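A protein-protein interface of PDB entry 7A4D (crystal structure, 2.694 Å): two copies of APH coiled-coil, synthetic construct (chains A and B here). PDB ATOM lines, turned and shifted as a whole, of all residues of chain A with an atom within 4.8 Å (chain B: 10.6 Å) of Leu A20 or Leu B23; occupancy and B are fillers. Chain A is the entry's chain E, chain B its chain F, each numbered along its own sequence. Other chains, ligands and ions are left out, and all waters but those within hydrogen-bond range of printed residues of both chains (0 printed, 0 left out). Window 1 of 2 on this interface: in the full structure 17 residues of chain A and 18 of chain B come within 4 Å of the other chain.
Ile A16 touches Leu B23 (CG2 to CD2, 3.7 Å). CG2 of Ile A16 touches CB of Ala B27, 3.6 Å away. Leu A20 touches Leu B20 (O to CD2, 3.7 Å). Leu B23 touches Leu A20 (CB to CD2, 3.6 Å). Leu A20 touches Gln B24 (CD2 to N, 3.7 Å). Leu A23 touches Ile B16. Leu A23 touches Leu B20 (CB to CD2, 3.4 Å). N of Gln A24 touches CD2 of Leu B20 (3.9 Å).
Of chain B, only Leu B23 (3.7 Å) and Ala B27 (3.6 Å) come within 4 Å of Ile A16. Leu A20 touches just these residues of chain B: Leu B20 (3.7 Å), Leu B23 (3.6 Å) and Gln B24 (3.7 Å). Gln A24 touches just one residue of chain B: Leu B20. Of the printed residues of chain A, Ile B16 touches Leu A23 (3.7 Å). Printed residues of chain A within 4 Å of Leu B20: Leu A20 (3.7 Å), Leu A23 (3.4 Å) and Gln A24 (3.9 Å). Leu B23 touches just these residues of chain A: Ile A16 and Leu A20. Of the printed residues of chain A, Gln B24 touches Leu A20. Printed residues of chain A within 4 Å of Ala B27: Ile A16. The nearest printed residue of chain A that does not touch Leu B20 is Gln A19 (5.0 Å).
Hydrophobic or aromatic side chains of chain A that line the printed part of chain B: Ile A16, Leu A20 and Leu A23. Of the 17 printed residues of chain B, 5 touch a printed residue of chain A. Hydrophobic or aromatic side chains of chain B within 4 Å of the printed part of chain A: Ile B16, Leu B20, Leu B23 and Ala B27.
Ile A16 touches Leu B23, and with the chains exchanged Leu A23 touches Ile B16. Leu B20 touches its own counterpart, Leu A20. Leu A20 touches Leu B23, and with the chains exchanged Leu A23 touches Leu B20. Leu A20 touches Gln B24, and with the chains exchanged Gln A24 touches Leu B20. Of the 8 pairs that touch across the chains among the printed residues, 7 have their exchanged pair printed and touching as well.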
ATOM      1  N   ILE A  16      18.977  24.277 -16.679  1.00  0.00           N
ATOM      2  CA  ILE A  16      19.680  24.005 -17.921  1.00  0.00           C
ATOM      3  C   ILE A  16      20.658  25.133 -18.214  1.00  0.00           C
ATOM      4  O   ILE A  16      21.823  24.893 -18.560  1.00  0.00           O
ATOM      5  CB  ILE A  16      18.679  23.785 -19.069  1.00  0.00           C
ATOM      6  CG1 ILE A  16      17.900  22.497 -18.867  1.00  0.00           C
ATOM      7  CG2 ILE A  16      19.362  23.751 -20.445  1.00  0.00           C
ATOM      8  CD1 ILE A  16      16.676  22.430 -19.780  1.00  0.00           C
ATOM      9  N   GLU A  17      20.224  26.377 -18.019  1.00  0.00           N
ATOM     10  CA  GLU A  17      21.119  27.505 -18.248  1.00  0.00           C
ATOM     11  C   GLU A  17      22.361  27.388 -17.384  1.00  0.00           C
ATOM     12  O   GLU A  17      23.475  27.663 -17.851  1.00  0.00           O
ATOM     13  CB  GLU A  17      20.390  28.810 -17.966  1.00  0.00           C
ATOM     14  CG  GLU A  17      19.246  29.050 -18.905  1.00  0.00           C
ATOM     15  CD  GLU A  17      18.569  30.369 -18.673  1.00  0.00           C
ATOM     16  OE1 GLU A  17      18.810  30.998 -17.619  1.00  0.00           O
ATOM     17  OE2 GLU A  17      17.788  30.783 -19.552  1.00  0.00           O
ATOM     18  N   GLU A  18      22.188  26.935 -16.129  1.00  0.00           N
ATOM     19  CA  GLU A  18      23.315  26.767 -15.218  1.00  0.00           C
ATOM     20  C   GLU A  18      24.288  25.717 -15.730  1.00  0.00           C
ATOM     21  O   GLU A  18      25.504  25.934 -15.711  1.00  0.00           O
ATOM     22  CB  GLU A  18      22.804  26.385 -13.831  1.00  0.00           C
ATOM     23  CG  GLU A  18      22.138  27.508 -13.029  1.00  0.00           C
ATOM     24  CD  GLU A  18      23.111  28.579 -12.592  1.00  0.00           C
ATOM     25  OE1 GLU A  18      22.693  29.752 -12.494  1.00  0.00           O
ATOM     26  OE2 GLU A  18      24.294  28.253 -12.355  1.00  0.00           O
ATOM     27  N   GLN A  19      23.778  24.592 -16.244  1.00  0.00           N
ATOM     28  CA  GLN A  19      24.672  23.577 -16.801  1.00  0.00           C
ATOM     29  C   GLN A  19      25.381  24.091 -18.047  1.00  0.00           C
ATOM     30  O   GLN A  19      26.568  23.809 -18.246  1.00  0.00           O
ATOM     31  CB  GLN A  19      23.904  22.315 -17.188  1.00  0.00           C
ATOM     32  CG  GLN A  19      23.549  21.456 -16.079  1.00  0.00           C
ATOM     33  CD  GLN A  19      24.493  20.323 -15.969  1.00  0.00           C
ATOM     34  OE1 GLN A  19      25.411  20.219 -16.770  1.00  0.00           O
ATOM     35  NE2 GLN A  19      24.287  19.457 -14.971  1.00  0.00           N
ATOM     36  N   LEU A  20      24.680  24.866 -18.885  1.00  0.00           N
ATOM     37  CA  LEU A  20      25.335  25.473 -20.039  1.00  0.00           C
ATOM     38  C   LEU A  20      26.542  26.284 -19.602  1.00  0.00           C
ATOM     39  O   LEU A  20      27.658  26.046 -20.074  1.00  0.00           O
ATOM     40  CB  LEU A  20      24.336  26.327 -20.811  1.00  0.00           C
ATOM     41  CG  LEU A  20      23.400  25.507 -21.699  1.00  0.00           C
ATOM     42  CD1 LEU A  20      22.211  26.327 -22.172  1.00  0.00           C
ATOM     43  CD2 LEU A  20      24.214  25.038 -22.884  1.00  0.00           C
ATOM     44  N   ALA A  21      26.345  27.206 -18.647  1.00  0.00           N
ATOM     45  CA  ALA A  21      27.454  27.985 -18.095  1.00  0.00           C
ATOM     46  C   ALA A  21      28.553  27.073 -17.560  1.00  0.00           C
ATOM     47  O   ALA A  21      29.736  27.278 -17.852  1.00  0.00           O
ATOM     48  CB  ALA A  21      26.950  28.929 -17.006  1.00  0.00           C
ATOM     49  N   GLN A  22      28.182  26.049 -16.779  1.00  0.00           N
ATOM     50  CA  GLN A  22      29.196  25.149 -16.240  1.00  0.00           C
ATOM     51  C   GLN A  22      29.976  24.450 -17.349  1.00  0.00           C
ATOM     52  O   GLN A  22      31.205  24.349 -17.285  1.00  0.00           O
ATOM     53  CB  GLN A  22      28.556  24.109 -15.327  1.00  0.00           C
ATOM     54  CG  GLN A  22      29.570  23.114 -14.752  1.00  0.00           C
ATOM     55  CD  GLN A  22      29.007  22.124 -13.723  1.00  0.00           C
ATOM     56  OE1 GLN A  22      27.883  21.617 -13.840  1.00  0.00           O
ATOM     57  NE2 GLN A  22      29.795  21.870 -12.691  1.00  0.00           N
ATOM     58  N   LEU A  23      29.282  23.963 -18.382  1.00  0.00           N
ATOM     59  CA  LEU A  23      29.977  23.297 -19.480  1.00  0.00           C
ATOM     60  C   LEU A  23      30.783  24.298 -20.294  1.00  0.00           C
ATOM     61  O   LEU A  23      31.921  24.017 -20.708  1.00  0.00           O
ATOM     62  CB  LEU A  23      28.982  22.573 -20.371  1.00  0.00           C
ATOM     63  CG  LEU A  23      28.890  21.091 -20.098  1.00  0.00           C
ATOM     64  CD1 LEU A  23      27.865  20.487 -21.048  1.00  0.00           C
ATOM     65  CD2 LEU A  23      30.264  20.465 -20.237  1.00  0.00           C
ATOM     66  N   GLN A  24      30.224  25.485 -20.512  1.00  0.00           N
ATOM     67  CA  GLN A  24      31.037  26.528 -21.107  1.00  0.00           C
ATOM     68  C   GLN A  24      32.371  26.635 -20.374  1.00  0.00           C
ATOM     69  O   GLN A  24      33.436  26.555 -20.998  1.00  0.00           O
ATOM     70  CB  GLN A  24      30.293  27.866 -21.088  1.00  0.00           C
ATOM     71  CG  GLN A  24      29.225  27.975 -22.153  1.00  0.00           C
ATOM     72  CD  GLN A  24      28.772  29.393 -22.341  1.00  0.00           C
ATOM     73  OE1 GLN A  24      29.593  30.309 -22.336  1.00  0.00           O
ATOM     74  NE2 GLN A  24      27.493  29.589 -22.585  1.00  0.00           N
ATOM     75  N   ALA B  15      33.470  16.543 -27.974  1.00  0.00           N
ATOM     76  CA  ALA B  15      32.282  16.005 -27.311  1.00  0.00           C
ATOM     77  C   ALA B  15      31.626  17.044 -26.406  1.00  0.00           C
ATOM     78  O   ALA B  15      30.388  17.105 -26.311  1.00  0.00           O
ATOM     79  CB  ALA B  15      32.636  14.752 -26.507  1.00  0.00           C
ATOM     80  N   ILE B  16      32.432  17.881 -25.742  1.00  0.00           N
ATOM     81  CA  ILE B  16      31.847  18.895 -24.868  1.00  0.00           C
ATOM     82  C   ILE B  16      31.114  19.944 -25.695  1.00  0.00           C
ATOM     83  O   ILE B  16      29.974  20.307 -25.391  1.00  0.00           O
ATOM     84  CB  ILE B  16      32.939  19.507 -23.968  1.00  0.00           C
ATOM     85  CG1 ILE B  16      33.437  18.443 -22.989  1.00  0.00           C
ATOM     86  CG2 ILE B  16      32.412  20.707 -23.203  1.00  0.00           C
ATOM     87  CD1 ILE B  16      34.750  18.766 -22.347  1.00  0.00           C
ATOM     88  N   GLU B  17      31.732  20.405 -26.780  1.00  0.00           N
ATOM     89  CA  GLU B  17      31.073  21.356 -27.673  1.00  0.00           C
ATOM     90  C   GLU B  17      29.796  20.763 -28.245  1.00  0.00           C
ATOM     91  O   GLU B  17      28.798  21.472 -28.418  1.00  0.00           O
ATOM     92  CB  GLU B  17      32.033  21.784 -28.797  1.00  0.00           C
ATOM     93  CG  GLU B  17      33.291  22.512 -28.305  1.00  0.00           C
ATOM     94  CD  GLU B  17      34.150  23.013 -29.428  1.00  0.00           C
ATOM     95  OE1 GLU B  17      33.900  22.615 -30.582  1.00  0.00           O
ATOM     96  OE2 GLU B  17      35.092  23.786 -29.164  1.00  0.00           O
ATOM     97  N   GLU B  18      29.814  19.463 -28.560  1.00  0.00           N
ATOM     98  CA  GLU B  18      28.605  18.801 -29.043  1.00  0.00           C
ATOM     99  C   GLU B  18      27.502  18.797 -27.985  1.00  0.00           C
ATOM    100  O   GLU B  18      26.340  19.113 -28.290  1.00  0.00           O
ATOM    101  CB  GLU B  18      28.925  17.370 -29.466  1.00  0.00           C
ATOM    102  CG  GLU B  18      29.709  17.278 -30.758  1.00  0.00           C
ATOM    103  CD  GLU B  18      28.907  17.723 -31.957  1.00  0.00           C
ATOM    104  OE1 GLU B  18      29.515  18.272 -32.906  1.00  0.00           O
ATOM    105  OE2 GLU B  18      27.665  17.528 -31.937  1.00  0.00           O
ATOM    106  N   GLN B  19      27.846  18.509 -26.719  1.00  0.00           N
ATOM    107  CA  GLN B  19      26.799  18.530 -25.706  1.00  0.00           C
ATOM    108  C   GLN B  19      26.297  19.937 -25.425  1.00  0.00           C
ATOM    109  O   GLN B  19      25.099  20.118 -25.153  1.00  0.00           O
ATOM    110  CB  GLN B  19      27.245  17.911 -24.400  1.00  0.00           C
ATOM    111  CG  GLN B  19      26.021  17.398 -23.656  1.00  0.00           C
ATOM    112  CD  GLN B  19      26.342  16.275 -22.733  1.00  0.00           C
ATOM    113  OE1 GLN B  19      26.405  15.105 -23.140  1.00  0.00           O
ATOM    114  NE2 GLN B  19      26.555  16.613 -21.460  1.00  0.00           N
ATOM    115  N   LEU B  20      27.177  20.943 -25.492  1.00  0.00           N
ATOM    116  CA  LEU B  20      26.695  22.311 -25.386  1.00  0.00           C
ATOM    117  C   LEU B  20      25.605  22.591 -26.418  1.00  0.00           C
ATOM    118  O   LEU B  20      24.533  23.106 -26.074  1.00  0.00           O
ATOM    119  CB  LEU B  20      27.847  23.298 -25.531  1.00  0.00           C
ATOM    120  CG  LEU B  20      28.644  23.440 -24.248  1.00  0.00           C
ATOM    121  CD1 LEU B  20      29.927  24.253 -24.498  1.00  0.00           C
ATOM    122  CD2 LEU B  20      27.765  24.020 -23.143  1.00  0.00           C
ATOM    123  N   ALA B  21      25.862  22.267 -27.694  1.00  0.00           N
ATOM    124  CA  ALA B  21      24.840  22.462 -28.720  1.00  0.00           C
ATOM    125  C   ALA B  21      23.555  21.741 -28.345  1.00  0.00           C
ATOM    126  O   ALA B  21      22.462  22.322 -28.404  1.00  0.00           O
ATOM    127  CB  ALA B  21      25.340  21.989 -30.089  1.00  0.00           C
ATOM    128  N   GLN B  22      23.671  20.468 -27.946  1.00  0.00           N
ATOM    129  CA  GLN B  22      22.491  19.700 -27.556  1.00  0.00           C
ATOM    130  C   GLN B  22      21.757  20.343 -26.380  1.00  0.00           C
ATOM    131  O   GLN B  22      20.520  20.357 -26.345  1.00  0.00           O
ATOM    132  CB  GLN B  22      22.905  18.275 -27.222  1.00  0.00           C
ATOM    133  CG  GLN B  22      21.786  17.390 -26.756  1.00  0.00           C
ATOM    134  CD  GLN B  22      22.236  15.973 -26.564  1.00  0.00           C
ATOM    135  OE1 GLN B  22      23.366  15.724 -26.156  1.00  0.00           O
ATOM    136  NE2 GLN B  22      21.352  15.028 -26.850  1.00  0.00           N
ATOM    137  N   LEU B  23      22.498  20.844 -25.389  1.00  0.00           N
ATOM    138  CA  LEU B  23      21.853  21.501 -24.255  1.00  0.00           C
ATOM    139  C   LEU B  23      21.243  22.842 -24.647  1.00  0.00           C
ATOM    140  O   LEU B  23      20.170  23.206 -24.154  1.00  0.00           O
ATOM    141  CB  LEU B  23      22.847  21.706 -23.122  1.00  0.00           C
ATOM    142  CG  LEU B  23      22.723  20.692 -22.027  1.00  0.00           C
ATOM    143  CD1 LEU B  23      23.779  21.065 -21.065  1.00  0.00           C
ATOM    144  CD2 LEU B  23      21.351  20.783 -21.410  1.00  0.00           C
ATOM    145  N   GLN B  24      21.927  23.615 -25.489  1.00  0.00           N
ATOM    146  CA  GLN B  24      21.326  24.850 -25.976  1.00  0.00           C
ATOM    147  C   GLN B  24      19.961  24.578 -26.570  1.00  0.00           C
ATOM    148  O   GLN B  24      18.966  25.206 -26.195  1.00  0.00           O
ATOM    149  CB  GLN B  24      22.217  25.506 -27.027  1.00  0.00           C
ATOM    150  CG  GLN B  24      23.426  26.172 -26.454  1.00  0.00           C
ATOM    151  CD  GLN B  24      24.138  27.029 -27.460  1.00  0.00           C
ATOM    152  OE1 GLN B  24      23.510  27.767 -28.207  1.00  0.00           O
ATOM    153  NE2 GLN B  24      25.462  26.932 -27.491  1.00  0.00           N
ATOM    154  N   TRP B  25      19.897  23.602 -27.475  1.00  0.00           N
ATOM    155  CA  TRP B  25      18.636  23.281 -28.125  1.00  0.00           C
ATOM    156  C   TRP B  25      17.611  22.839 -27.099  1.00  0.00           C
ATOM    157  O   TRP B  25      16.426  23.181 -27.203  1.00  0.00           O
ATOM    158  CB  TRP B  25      18.860  22.221 -29.201  1.00  0.00           C
ATOM    159  CG  TRP B  25      17.634  21.873 -30.005  1.00  0.00           C
ATOM    160  CD1 TRP B  25      16.927  20.711 -29.943  1.00  0.00           C
ATOM    161  CD2 TRP B  25      16.978  22.691 -30.996  1.00  0.00           C
ATOM    162  NE1 TRP B  25      15.872  20.755 -30.812  1.00  0.00           N
ATOM    163  CE2 TRP B  25      15.879  21.952 -31.476  1.00  0.00           C
ATOM    164  CE3 TRP B  25      17.215  23.968 -31.523  1.00  0.00           C
ATOM    165  CZ2 TRP B  25      15.014  22.446 -32.452  1.00  0.00           C
ATOM    166  CZ3 TRP B  25      16.353  24.462 -32.494  1.00  0.00           C
ATOM    167  CH2 TRP B  25      15.266  23.700 -32.947  1.00  0.00           C
ATOM    168  N   LYS B  26      18.057  22.100 -26.079  1.00  0.00           N
ATOM    169  CA  LYS B  26      17.148  21.686 -25.019  1.00  0.00           C
ATOM    170  C   LYS B  26      16.549  22.900 -24.314  1.00  0.00           C
ATOM    171  O   LYS B  26      15.335  22.974 -24.089  1.00  0.00           O
ATOM    172  CB  LYS B  26      17.890  20.788 -24.037  1.00  0.00           C
ATOM    173  CG  LYS B  26      16.990  19.776 -23.394  1.00  0.00           C
ATOM    174  CD  LYS B  26      16.635  18.750 -24.426  1.00  0.00           C
ATOM    175  CE  LYS B  26      15.451  17.917 -23.993  1.00  0.00           C
ATOM    176  NZ  LYS B  26      15.266  16.741 -24.910  1.00  0.00           N
ATOM    177  N   ALA B  27      17.386  23.870 -23.959  1.00  0.00           N
ATOM    178  CA  ALA B  27      16.877  25.089 -23.337  1.00  0.00           C
ATOM    179  C   ALA B  27      15.886  25.808 -24.251  1.00  0.00           C
ATOM    180  O   ALA B  27      14.819  26.252 -23.806  1.00  0.00           O
ATOM    181  CB  ALA B  27      18.039  26.007 -22.954  1.00  0.00           C
ATOM    182  N   GLN B  28      16.242  25.973 -25.527  1.00  0.00           N
ATOM    183  CA  GLN B  28      15.327  26.629 -26.453  1.00  0.00           C
ATOM    184  C   GLN B  28      13.981  25.925 -26.476  1.00  0.00           C
ATOM    185  O   GLN B  28      12.928  26.564 -26.376  1.00  0.00           O
ATOM    186  CB  GLN B  28      15.921  26.667 -27.862  1.00  0.00           C
ATOM    187  CG  GLN B  28      15.013  27.334 -28.876  1.00  0.00           C
ATOM    188  CD  GLN B  28      14.698  28.767 -28.534  1.00  0.00           C
ATOM    189  OE1 GLN B  28      15.550  29.506 -28.040  1.00  0.00           O
ATOM    190  NE2 GLN B  28      13.463  29.165 -28.772  1.00  0.00           N
ATOM    191  N   ALA B  29      14.000  24.598 -26.557  1.00  0.00           N
ATOM    192  CA  ALA B  29      12.754  23.841 -26.604  1.00  0.00           C
ATOM    193  C   ALA B  29      11.957  24.043 -25.321  1.00  0.00           C
ATOM    194  O   ALA B  29      10.752  24.340 -25.352  1.00  0.00           O
ATOM    195  CB  ALA B  29      13.072  22.362 -26.816  1.00  0.00           C
ATOM    196  N   ARG B  30      12.641  23.940 -24.179  1.00  0.00           N
ATOM    197  CA  ARG B  30      12.000  24.130 -22.885  1.00  0.00           C
ATOM    198  C   ARG B  30      11.516  25.578 -22.731  1.00  0.00           C
ATOM    199  O   ARG B  30      10.413  25.816 -22.221  1.00  0.00           O
ATOM    200  CB  ARG B  30      13.005  23.725 -21.802  1.00  0.00           C
ATOM    201  CG  ARG B  30      12.502  22.959 -20.568  1.00  0.00           C
ATOM    202  CD  ARG B  30      11.456  21.876 -20.796  1.00  0.00           C
ATOM    203  NE  ARG B  30      11.925  20.658 -21.454  1.00  0.00           N
ATOM    204  CZ  ARG B  30      12.505  19.635 -20.842  1.00  0.00           C
ATOM    205  NH1 ARG B  30      12.721  19.679 -19.537  1.00  0.00           N
ATOM    206  NH2 ARG B  30      12.881  18.569 -21.540  1.00  0.00           N
ATOM    207  N   LYS B  31      12.301  26.556 -23.217  1.00  0.00           N
ATOM    208  CA  LYS B  31      11.872  27.957 -23.209  1.00  0.00           C
ATOM    209  C   LYS B  31      10.566  28.157 -23.983  1.00  0.00           C
ATOM    210  O   LYS B  31       9.651  28.850 -23.522  1.00  0.00           O
ATOM    211  CB  LYS B  31      12.972  28.849 -23.792  1.00  0.00           C
ATOM    212  CG  LYS B  31      12.582  30.340 -23.944  1.00  0.00           C
ATOM    213  CD  LYS B  31      13.680  31.159 -24.671  1.00  0.00           C
ATOM    214  CE  LYS B  31      13.192  32.580 -24.882  1.00  0.00           C
ATOM    215  NZ  LYS B  31      14.180  33.585 -25.352  1.00  0.00           N
